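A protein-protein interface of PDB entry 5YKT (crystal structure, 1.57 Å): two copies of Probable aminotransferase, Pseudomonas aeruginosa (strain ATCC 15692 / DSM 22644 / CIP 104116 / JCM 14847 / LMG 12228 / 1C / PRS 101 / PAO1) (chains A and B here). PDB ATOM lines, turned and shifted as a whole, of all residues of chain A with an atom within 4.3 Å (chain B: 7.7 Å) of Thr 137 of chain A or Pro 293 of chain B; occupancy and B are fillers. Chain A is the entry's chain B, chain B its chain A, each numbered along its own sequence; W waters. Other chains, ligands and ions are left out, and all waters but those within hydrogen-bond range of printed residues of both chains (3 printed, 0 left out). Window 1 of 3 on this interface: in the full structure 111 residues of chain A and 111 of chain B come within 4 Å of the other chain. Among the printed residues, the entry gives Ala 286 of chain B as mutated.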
ATOM      1  N   THR A 136      11.187  23.868  22.554  1.00  0.00           N
ATOM      2  CA  THR A 136      12.378  24.379  23.254  1.00  0.00           C
ATOM      3  C   THR A 136      13.579  23.453  22.989  1.00  0.00           C
ATOM      4  O   THR A 136      13.460  22.457  22.275  1.00  0.00           O
ATOM      5  CB  THR A 136      12.145  24.455  24.770  1.00  0.00           C
ATOM      6  OG1 THR A 136      12.030  23.135  25.293  1.00  0.00           O
ATOM      7  CG2 THR A 136      10.905  25.238  25.091  1.00  0.00           C
ATOM      8  N   THR A 137      14.731  23.768  23.580  1.00  0.00           N
ATOM      9  CA  THR A 137      15.901  22.889  23.449  1.00  0.00           C
ATOM     10  C   THR A 137      16.065  21.909  24.616  1.00  0.00           C
ATOM     11  O   THR A 137      17.009  21.131  24.611  1.00  0.00           O
ATOM     12  CB  THR A 137      17.186  23.702  23.242  1.00  0.00           C
ATOM     13  OG1 THR A 137      17.361  24.657  24.300  1.00  0.00           O
ATOM     14  CG2 THR A 137      17.129  24.455  21.902  1.00  0.00           C
ATOM     15  N   SER A 138      15.142  21.925  25.584  1.00  0.00           N
ATOM     16  CA  SER A 138      15.170  20.957  26.682  1.00  0.00           C
ATOM     17  C   SER A 138      13.883  20.943  27.470  1.00  0.00           C
ATOM     18  O   SER A 138      13.146  21.933  27.509  1.00  0.00           O
ATOM     19  CB  SER A 138      16.316  21.272  27.656  1.00  0.00           C
ATOM     20  OG  SER A 138      16.040  22.452  28.394  1.00  0.00           O
ATOM     21  N   ASP A 141      13.830  23.718  29.974  1.00  0.00           N
ATOM     22  CA  ASP A 141      13.393  25.001  29.425  1.00  0.00           C
ATOM     23  C   ASP A 141      11.898  25.051  29.193  1.00  0.00           C
ATOM     24  O   ASP A 141      11.282  26.078  29.455  1.00  0.00           O
ATOM     25  CB  ASP A 141      14.130  25.320  28.137  1.00  0.00           C
ATOM     26  CG  ASP A 141      15.541  25.769  28.375  1.00  0.00           C
ATOM     27  OD1 ASP A 141      15.988  25.896  29.538  1.00  0.00           O
ATOM     28  OD2 ASP A 141      16.212  26.018  27.352  1.00  0.00           O
ATOM     29  N   ILE A 292      18.808  14.986  19.319  1.00  0.00           N
ATOM     30  CA  ILE A 292      18.924  16.429  19.209  1.00  0.00           C
ATOM     31  C   ILE A 292      18.211  17.001  20.449  1.00  0.00           C
ATOM     32  O   ILE A 292      17.032  16.707  20.676  1.00  0.00           O
ATOM     33  CB  ILE A 292      18.243  16.962  17.948  1.00  0.00           C
ATOM     34  CG1 ILE A 292      18.848  16.318  16.698  1.00  0.00           C
ATOM     35  CG2 ILE A 292      18.367  18.479  17.867  1.00  0.00           C
ATOM     36  CD1 ILE A 292      17.912  16.397  15.554  1.00  0.00           C
ATOM     37  N   PRO A 293      18.924  17.798  21.264  1.00  0.00           N
ATOM     38  CA  PRO A 293      18.281  18.408  22.437  1.00  0.00           C
ATOM     39  C   PRO A 293      17.004  19.138  22.035  1.00  0.00           C
ATOM     40  O   PRO A 293      17.033  20.018  21.159  1.00  0.00           O
ATOM     41  CB  PRO A 293      19.344  19.349  22.974  1.00  0.00           C
ATOM     42  CG  PRO A 293      20.640  18.715  22.554  1.00  0.00           C
ATOM     43  CD  PRO A 293      20.370  18.105  21.211  1.00  0.00           C
ATOM     44  N   SER A 294      15.890  18.746  22.647  1.00  0.00           N
ATOM     45  CA  SER A 294      14.584  19.242  22.263  1.00  0.00           C
ATOM     46  C   SER A 294      13.571  18.983  23.351  1.00  0.00           C
ATOM     47  O   SER A 294      13.757  18.109  24.192  1.00  0.00           O
ATOM     48  CB  SER A 294      14.061  18.525  21.013  1.00  0.00           C
ATOM     49  OG  SER A 294      14.969  18.472  19.936  1.00  0.00           O
ATOM     50  N   LEU A 329      18.188  28.381  19.101  1.00  0.00           N
ATOM     51  CA  LEU A 329      18.071  27.157  18.293  1.00  0.00           C
ATOM     52  C   LEU A 329      16.769  26.400  18.560  1.00  0.00           C
ATOM     53  O   LEU A 329      16.581  25.294  18.048  1.00  0.00           O
ATOM     54  CB  LEU A 329      19.293  26.243  18.489  1.00  0.00           C
ATOM     55  CG  LEU A 329      20.464  26.604  17.567  1.00  0.00           C
ATOM     56  CD1 LEU A 329      21.159  27.876  18.000  1.00  0.00           C
ATOM     57  CD2 LEU A 329      21.435  25.449  17.485  1.00  0.00           C
ATOM     58  N   ALA A 330      15.873  26.978  19.358  1.00  0.00           N
ATOM     59  CA  ALA A 330      14.592  26.348  19.649  1.00  0.00           C
ATOM     60  C   ALA A 330      13.696  26.301  18.415  1.00  0.00           C
ATOM     61  O   ALA A 330      13.559  27.283  17.681  1.00  0.00           O
ATOM     62  CB  ALA A 330      13.882  27.078  20.776  1.00  0.00           C
ATOM     63  N   GLN A 335      15.487  19.771  14.559  1.00  0.00           N
ATOM     64  CA  GLN A 335      14.602  19.220  15.578  1.00  0.00           C
ATOM     65  C   GLN A 335      13.286  18.741  14.961  1.00  0.00           C
ATOM     66  O   GLN A 335      12.787  17.662  15.266  1.00  0.00           O
ATOM     67  CB  GLN A 335      14.275  20.285  16.629  1.00  0.00           C
ATOM     68  CG  GLN A 335      15.405  20.714  17.540  1.00  0.00           C
ATOM     69  CD  GLN A 335      14.921  21.782  18.485  1.00  0.00           C
ATOM     70  OE1 GLN A 335      14.221  22.709  18.078  1.00  0.00           O
ATOM     71  NE2 GLN A 335      15.230  21.628  19.780  1.00  0.00           N
ATOM     72  N   VAL B 135      30.071  20.877  28.593  1.00  0.00           N
ATOM     73  CA  VAL B 135      29.135  21.100  27.500  1.00  0.00           C
ATOM     74  C   VAL B 135      27.718  21.227  28.044  1.00  0.00           C
ATOM     75  O   VAL B 135      27.335  20.498  28.966  1.00  0.00           O
ATOM     76  CB  VAL B 135      29.186  19.936  26.492  1.00  0.00           C
ATOM     77  CG1 VAL B 135      28.248  20.170  25.321  1.00  0.00           C
ATOM     78  CG2 VAL B 135      30.595  19.732  25.984  1.00  0.00           C
ATOM     79  N   THR B 136      26.923  22.124  27.450  1.00  0.00           N
ATOM     80  CA  THR B 136      25.492  22.259  27.768  1.00  0.00           C
ATOM     81  C   THR B 136      24.662  22.192  26.474  1.00  0.00           C
ATOM     82  O   THR B 136      25.217  22.014  25.393  1.00  0.00           O
ATOM     83  CB  THR B 136      25.180  23.585  28.475  1.00  0.00           C
ATOM     84  OG1 THR B 136      25.395  24.651  27.543  1.00  0.00           O
ATOM     85  CG2 THR B 136      26.058  23.771  29.689  1.00  0.00           C
ATOM     86  N   THR B 137      23.341  22.330  26.582  1.00  0.00           N
ATOM     87  CA  THR B 137      22.495  22.360  25.397  1.00  0.00           C
ATOM     88  C   THR B 137      22.176  23.773  24.900  1.00  0.00           C
ATOM     89  O   THR B 137      21.469  23.916  23.908  1.00  0.00           O
ATOM     90  CB  THR B 137      21.205  21.551  25.588  1.00  0.00           C
ATOM     91  OG1 THR B 137      20.493  22.027  26.728  1.00  0.00           O
ATOM     92  CG2 THR B 137      21.524  20.070  25.795  1.00  0.00           C
ATOM     93  N   SER B 138      22.703  24.805  25.565  1.00  0.00           N
ATOM     94  CA  SER B 138      22.508  26.181  25.107  1.00  0.00           C
ATOM     95  C   SER B 138      23.458  27.144  25.810  1.00  0.00           C
ATOM     96  O   SER B 138      23.904  26.892  26.933  1.00  0.00           O
ATOM     97  CB  SER B 138      21.084  26.662  25.358  1.00  0.00           C
ATOM     98  OG  SER B 138      20.843  26.835  26.749  1.00  0.00           O
ATOM     99  N   ALA B 139      23.715  28.270  25.164  1.00  0.00           N
ATOM    100  CA  ALA B 139      24.511  29.319  25.796  1.00  0.00           C
ATOM    101  C   ALA B 139      23.824  29.851  27.049  1.00  0.00           C
ATOM    102  O   ALA B 139      24.488  30.155  28.037  1.00  0.00           O
ATOM    103  CB  ALA B 139      24.790  30.456  24.825  1.00  0.00           C
ATOM    104  N   THR B 140      22.494  29.954  27.028  1.00  0.00           N
ATOM    105  CA  THR B 140      21.752  30.329  28.235  1.00  0.00           C
ATOM    106  C   THR B 140      22.141  29.428  29.398  1.00  0.00           C
ATOM    107  O   THR B 140      22.474  29.913  30.502  1.00  0.00           O
ATOM    108  CB  THR B 140      20.230  30.251  28.032  1.00  0.00           C
ATOM    109  OG1 THR B 140      19.795  31.275  27.108  1.00  0.00           O
ATOM    110  CG2 THR B 140      19.505  30.394  29.346  1.00  0.00           C
ATOM    111  N   ASP B 141      22.104  28.118  29.156  1.00  0.00           N
ATOM    112  CA  ASP B 141      22.407  27.184  30.227  1.00  0.00           C
ATOM    113  C   ASP B 141      23.855  27.271  30.674  1.00  0.00           C
ATOM    114  O   ASP B 141      24.131  27.170  31.865  1.00  0.00           O
ATOM    115  CB  ASP B 141      22.080  25.753  29.804  1.00  0.00           C
ATOM    116  CG  ASP B 141      20.616  25.468  29.811  1.00  0.00           C
ATOM    117  OD1 ASP B 141      19.794  26.348  30.191  1.00  0.00           O
ATOM    118  OD2 ASP B 141      20.279  24.338  29.431  1.00  0.00           O
ATOM    119  N   GLY B 285      28.267  29.642  22.530  1.00  0.00           N
ATOM    120  CA  GLY B 285      27.040  28.958  22.115  1.00  0.00           C
ATOM    121  C   GLY B 285      27.062  28.078  20.871  1.00  0.00           C
ATOM    122  O   GLY B 285      28.095  27.520  20.483  1.00  0.00           O
ATOM    123  N   ALA B 286      25.897  27.927  20.243  1.00  0.00           N
ATOM    124  CA  ALA B 286      25.654  26.781  19.357  1.00  0.00           C
ATOM    125  C   ALA B 286      26.220  26.857  17.951  1.00  0.00           C
ATOM    126  O   ALA B 286      26.166  25.853  17.245  1.00  0.00           O
ATOM    127  CB  ALA B 286      24.165  26.486  19.295  1.00  0.00           C
ATOM    128  N   ALA B 289      28.170  23.544  16.703  1.00  0.00           N
ATOM    129  CA  ALA B 289      27.647  22.178  16.544  1.00  0.00           C
ATOM    130  C   ALA B 289      26.596  22.003  15.450  1.00  0.00           C
ATOM    131  O   ALA B 289      25.743  21.133  15.517  1.00  0.00           O
ATOM    132  CB  ALA B 289      27.109  21.665  17.879  1.00  0.00           C
ATOM    133  N   GLY B 290      26.690  22.822  14.407  1.00  0.00           N
ATOM    134  CA  GLY B 290      25.968  22.584  13.170  1.00  0.00           C
ATOM    135  C   GLY B 290      24.454  22.554  13.223  1.00  0.00           C
ATOM    136  O   GLY B 290      23.823  21.867  12.411  1.00  0.00           O
ATOM    137  N   GLY B 291      23.882  23.305  14.159  1.00  0.00           N
ATOM    138  CA  GLY B 291      22.429  23.292  14.367  1.00  0.00           C
ATOM    139  C   GLY B 291      21.927  22.368  15.449  1.00  0.00           C
ATOM    140  O   GLY B 291      20.729  22.323  15.733  1.00  0.00           O
ATOM    141  N   ILE B 292      22.823  21.605  16.062  1.00  0.00           N
ATOM    142  CA  ILE B 292      22.463  20.841  17.238  1.00  0.00           C
ATOM    143  C   ILE B 292      22.585  21.823  18.422  1.00  0.00           C
ATOM    144  O   ILE B 292      23.650  22.386  18.638  1.00  0.00           O
ATOM    145  CB  ILE B 292      23.393  19.655  17.476  1.00  0.00           C
ATOM    146  CG1 ILE B 292      23.396  18.722  16.258  1.00  0.00           C
ATOM    147  CG2 ILE B 292      22.983  18.890  18.728  1.00  0.00           C
ATOM    148  CD1 ILE B 292      24.611  17.880  16.230  1.00  0.00           C
ATOM    149  N   PRO B 293      21.494  22.023  19.182  1.00  0.00           N
ATOM    150  CA  PRO B 293      21.574  22.923  20.338  1.00  0.00           C
ATOM    151  C   PRO B 293      22.729  22.526  21.250  1.00  0.00           C
ATOM    152  O   PRO B 293      22.806  21.364  21.703  1.00  0.00           O
ATOM    153  CB  PRO B 293      20.219  22.746  21.011  1.00  0.00           C
ATOM    154  CG  PRO B 293      19.288  22.373  19.885  1.00  0.00           C
ATOM    155  CD  PRO B 293      20.112  21.528  18.966  1.00  0.00           C
ATOM    156  N   SER B 294      23.632  23.472  21.490  1.00  0.00           N
ATOM    157  CA  SER B 294      24.869  23.188  22.208  1.00  0.00           C
ATOM    158  C   SER B 294      25.503  24.462  22.712  1.00  0.00           C
ATOM    159  O   SER B 294      25.229  25.536  22.204  1.00  0.00           O
ATOM    160  CB  SER B 294      25.909  22.518  21.307  1.00  0.00           C
ATOM    161  OG  SER B 294      25.441  21.426  20.571  1.00  0.00           O
ATOM    162  N   ALA B 295      26.375  24.310  23.695  1.00  0.00           N
ATOM    163  CA  ALA B 295      27.290  25.366  24.092  1.00  0.00           C
ATOM    164  C   ALA B 295      28.395  24.719  24.874  1.00  0.00           C
ATOM    165  O   ALA B 295      28.248  23.582  25.348  1.00  0.00           O
ATOM    166  CB  ALA B 295      26.599  26.419  24.945  1.00  0.00           C
ATOM    167  N   LEU B 329      20.663  15.618  27.845  1.00  0.00           N
ATOM    168  CA  LEU B 329      21.282  15.495  26.537  1.00  0.00           C
ATOM    169  C   LEU B 329      22.532  16.371  26.400  1.00  0.00           C
ATOM    170  O   LEU B 329      23.115  16.451  25.319  1.00  0.00           O
ATOM    171  CB  LEU B 329      20.291  15.787  25.409  1.00  0.00           C
ATOM    172  CG  LEU B 329      19.445  14.588  24.998  1.00  0.00           C
ATOM    173  CD1 LEU B 329      18.397  14.264  26.034  1.00  0.00           C
ATOM    174  CD2 LEU B 329      18.825  14.821  23.636  1.00  0.00           C
ATOM    175  N   ALA B 330      22.966  17.006  27.489  1.00  0.00           N
ATOM    176  CA  ALA B 330      24.172  17.816  27.469  1.00  0.00           C
ATOM    177  C   ALA B 330      25.417  16.946  27.285  1.00  0.00           C
ATOM    178  O   ALA B 330      25.573  15.919  27.948  1.00  0.00           O
ATOM    179  CB  ALA B 330      24.296  18.633  28.753  1.00  0.00           C
ATOM    180  N   GLY B 331      26.305  17.371  26.404  1.00  0.00           N
ATOM    181  CA  GLY B 331      27.553  16.644  26.190  1.00  0.00           C
ATOM    182  C   GLY B 331      27.386  15.331  25.479  1.00  0.00           C
ATOM    183  O   GLY B 331      28.172  14.419  25.674  1.00  0.00           O
ATOM    184  N   ASN B 332      26.373  15.241  24.624  1.00  0.00           N
ATOM    185  CA  ASN B 332      26.098  13.995  23.943  1.00  0.00           C
ATOM    186  C   ASN B 332      26.963  13.762  22.711  1.00  0.00           C
ATOM    187  O   ASN B 332      27.646  14.678  22.202  1.00  0.00           O
ATOM    188  CB  ASN B 332      24.595  13.797  23.710  1.00  0.00           C
ATOM    189  CG  ASN B 332      24.012  14.563  22.550  1.00  0.00           C
ATOM    190  OD1 ASN B 332      24.678  14.943  21.592  1.00  0.00           O
ATOM    191  ND2 ASN B 332      22.685  14.704  22.589  1.00  0.00           N
ATOM    192  N   GLN B 335      26.483  16.060  19.611  1.00  0.00           N
ATOM    193  CA  GLN B 335      27.063  17.383  19.787  1.00  0.00           C
ATOM    194  C   GLN B 335      28.579  17.332  19.588  1.00  0.00           C
ATOM    195  O   GLN B 335      29.161  18.183  18.919  1.00  0.00           O
ATOM    196  CB  GLN B 335      26.791  17.915  21.190  1.00  0.00           C
ATOM    197  CG  GLN B 335      25.361  18.266  21.525  1.00  0.00           C
ATOM    198  CD  GLN B 335      25.271  18.714  22.962  1.00  0.00           C
ATOM    199  OE1 GLN B 335      25.853  18.088  23.860  1.00  0.00           O
ATOM    200  NE2 GLN B 335      24.581  19.834  23.194  1.00  0.00           N
ATOM    201  N   MET B 339      30.889  19.319  16.898  1.00  0.00           N
ATOM    202  CA  MET B 339      31.973  20.210  17.372  1.00  0.00           C
ATOM    203  C   MET B 339      33.325  19.852  16.794  1.00  0.00           C
ATOM    204  O   MET B 339      34.077  20.734  16.360  1.00  0.00           O
ATOM    205  CB  MET B 339      32.063  20.226  18.899  1.00  0.00           C
ATOM    206  CG  MET B 339      30.910  20.909  19.558  1.00  0.00           C
ATOM    207  SD  MET B 339      31.119  20.721  21.349  1.00  0.00           S
ATOM    208  CE  MET B 339      29.493  21.264  21.843  1.00  0.00           C
HETATM  209  O   HOH W   1      18.404  27.195  27.825  1.00  0.00           O
HETATM  210  O   HOH W   2      18.668  24.009  26.602  1.00  0.00           O
HETATM  211  O   HOH W   3      17.833  23.784  29.945  1.00  0.00           O
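CG of Pro 293 of chain B touches CG2 of Thr 137 of chain A, at 3.6 Å.
Asp 141 of chain B touches Asp 141 of chain A.
Ile 292 of chain A touches Pro 293 of chain B.
Ile 292 of chain A touches Leu 329 of chain B.
Pro 293 of chain A touches Thr 137 of chain B (CG to CG2, 3.6 Å).
Pro 293 of chain A touches Ile 292 of chain B (CD to CG2, 3.7 Å).
O of Pro 293 of chain A touches CG of Pro 293 of chain B, 3.5 Å away.
Leu 329 of chain B touches Pro 293 of chain A (CD2 to N, 3.8 Å).
Leu 329 of chain A touches Gly 291 of chain B.
Leu 329 of chain A touches Ile 292 of chain B.
Of the 10 printed residues of chain A, 5 touch a printed residue of chain B.
Hydrophobic or aromatic side chains of chain A within 4 Å of the printed part of chain B: Ile 292, Pro 293 and Leu 329.
Along chain A the printed residues that touch a printed residue of chain B span positions 137 to 329.
Hydrophobic or aromatic side chains of chain B that line the printed part of chain A: Ala 286, Ile 292, Pro 293 and Leu 329.
Among the printed residues, 12 pairs touch across the chains.
Among the printed residues, no Asp or Glu carboxylate lies within 4 Å of a Lys or Arg side-chain nitrogen of the other chain.
Of the printed residues of chain B, Thr 137 of chain A touches Pro 293 (3.6 Å).
Pro 293 of chain B touches just these residues of chain A: Thr 137, Ile 292, Pro 293 and Leu 329.
Of the printed residues of chain B, Leu 329 of chain A touches Ala 286 (3.4 Å), Gly 291 (3.7 Å), Ile 292 (3.9 Å) and Pro 293 (3.8 Å).
Of the printed residues of chain B, Ile 292 of chain A touches Pro 293 (3.7 Å) and Leu 329 (3.9 Å).
Printed residues of chain A within 4 Å of Ala 286 of chain B: Leu 329.
Printed residues of chain A within 4 Å of Gly 291 of chain B: Leu 329 (3.7 Å).
Printed residues of chain B within 4 Å of Asp 141 of chain A: Asp 141 (3.9 Å).
Gln 335 of chain B touches none of the printed residues of chain A.
Ser 294 of chain B touches none of the printed residues of chain A.
The nearest residue of chain B that does not touch Thr 137 of chain A is Thr 137 of chain B (4.2 Å).
The nearest printed residue of chain B that does not touch Leu 329 of chain A is Ser 294 of chain B (5.0 Å).
Thr 137 of chain A touches Pro 293 of chain B, and with the chains exchanged Pro 293 of chain A touches Thr 137 of chain B.
Ile 292 of chain A touches Pro 293 of chain B, and with the chains exchanged Pro 293 of chain A touches Ile 292 of chain B.
Pro 293 of chain A touches its own counterpart, Pro 293 of chain B.
Pro 293 of chain A touches Leu 329 of chain B, and with the chains exchanged Leu 329 of chain A touches Pro 293 of chain B.
O of Pro 293 of chain B lies within hydrogen-bond range of NE2 of Gln 335 of chain B (2.8 Å).
The backbone NH (N) of Ala 286 of chain B lies close to the backbone carbonyl oxygen (O) of Ser 294 of chain B, at 3.2 Å.
The backbone carbonyl oxygen (O) of Thr 137 of chain A lies within hydrogen-bond range of the backbone NH (N) of Ser 294 of chain A (3.3 Å).
N of Asp 141 of chain A lies within hydrogen-bond range of OG of Ser 138 of chain A (3.0 Å).
O of Ile 292 of chain A lies within hydrogen-bond range of OG of Ser 294 of chain A (2.8 Å).
The backbone carbonyl oxygen (O) of Pro 293 of chain A lies within hydrogen-bond range of the side-chain amide nitrogen (NE2) of Gln 335 of chain A (2.8 Å).
Water W1 lies within hydrogen-bond range of the side-chain carboxylate of Asp 141 of chain A (2.5 Å), the side-chain hydroxyl of Ser 138 of chain B (2.7 Å) and the side-chain carboxylate of Asp 141 of chain B (2.9 Å).
Water W3 lies within hydrogen-bond range of OD2 of Asp 141 of chain B (2.6 Å), OG of Ser 138 of chain A (2.7 Å) and OD1 of Asp 141 of chain A (2.8 Å).
Water W2 lies within hydrogen-bond range of the side-chain hydroxyl of Thr 137 of chain B (2.7 Å), the side-chain hydroxyl of Thr 137 of chain A (2.7 Å), the side-chain carboxylate of Asp 141 of chain A (3.3 Å) and the side-chain carboxylate of Asp 141 of chain B (3.3 Å).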
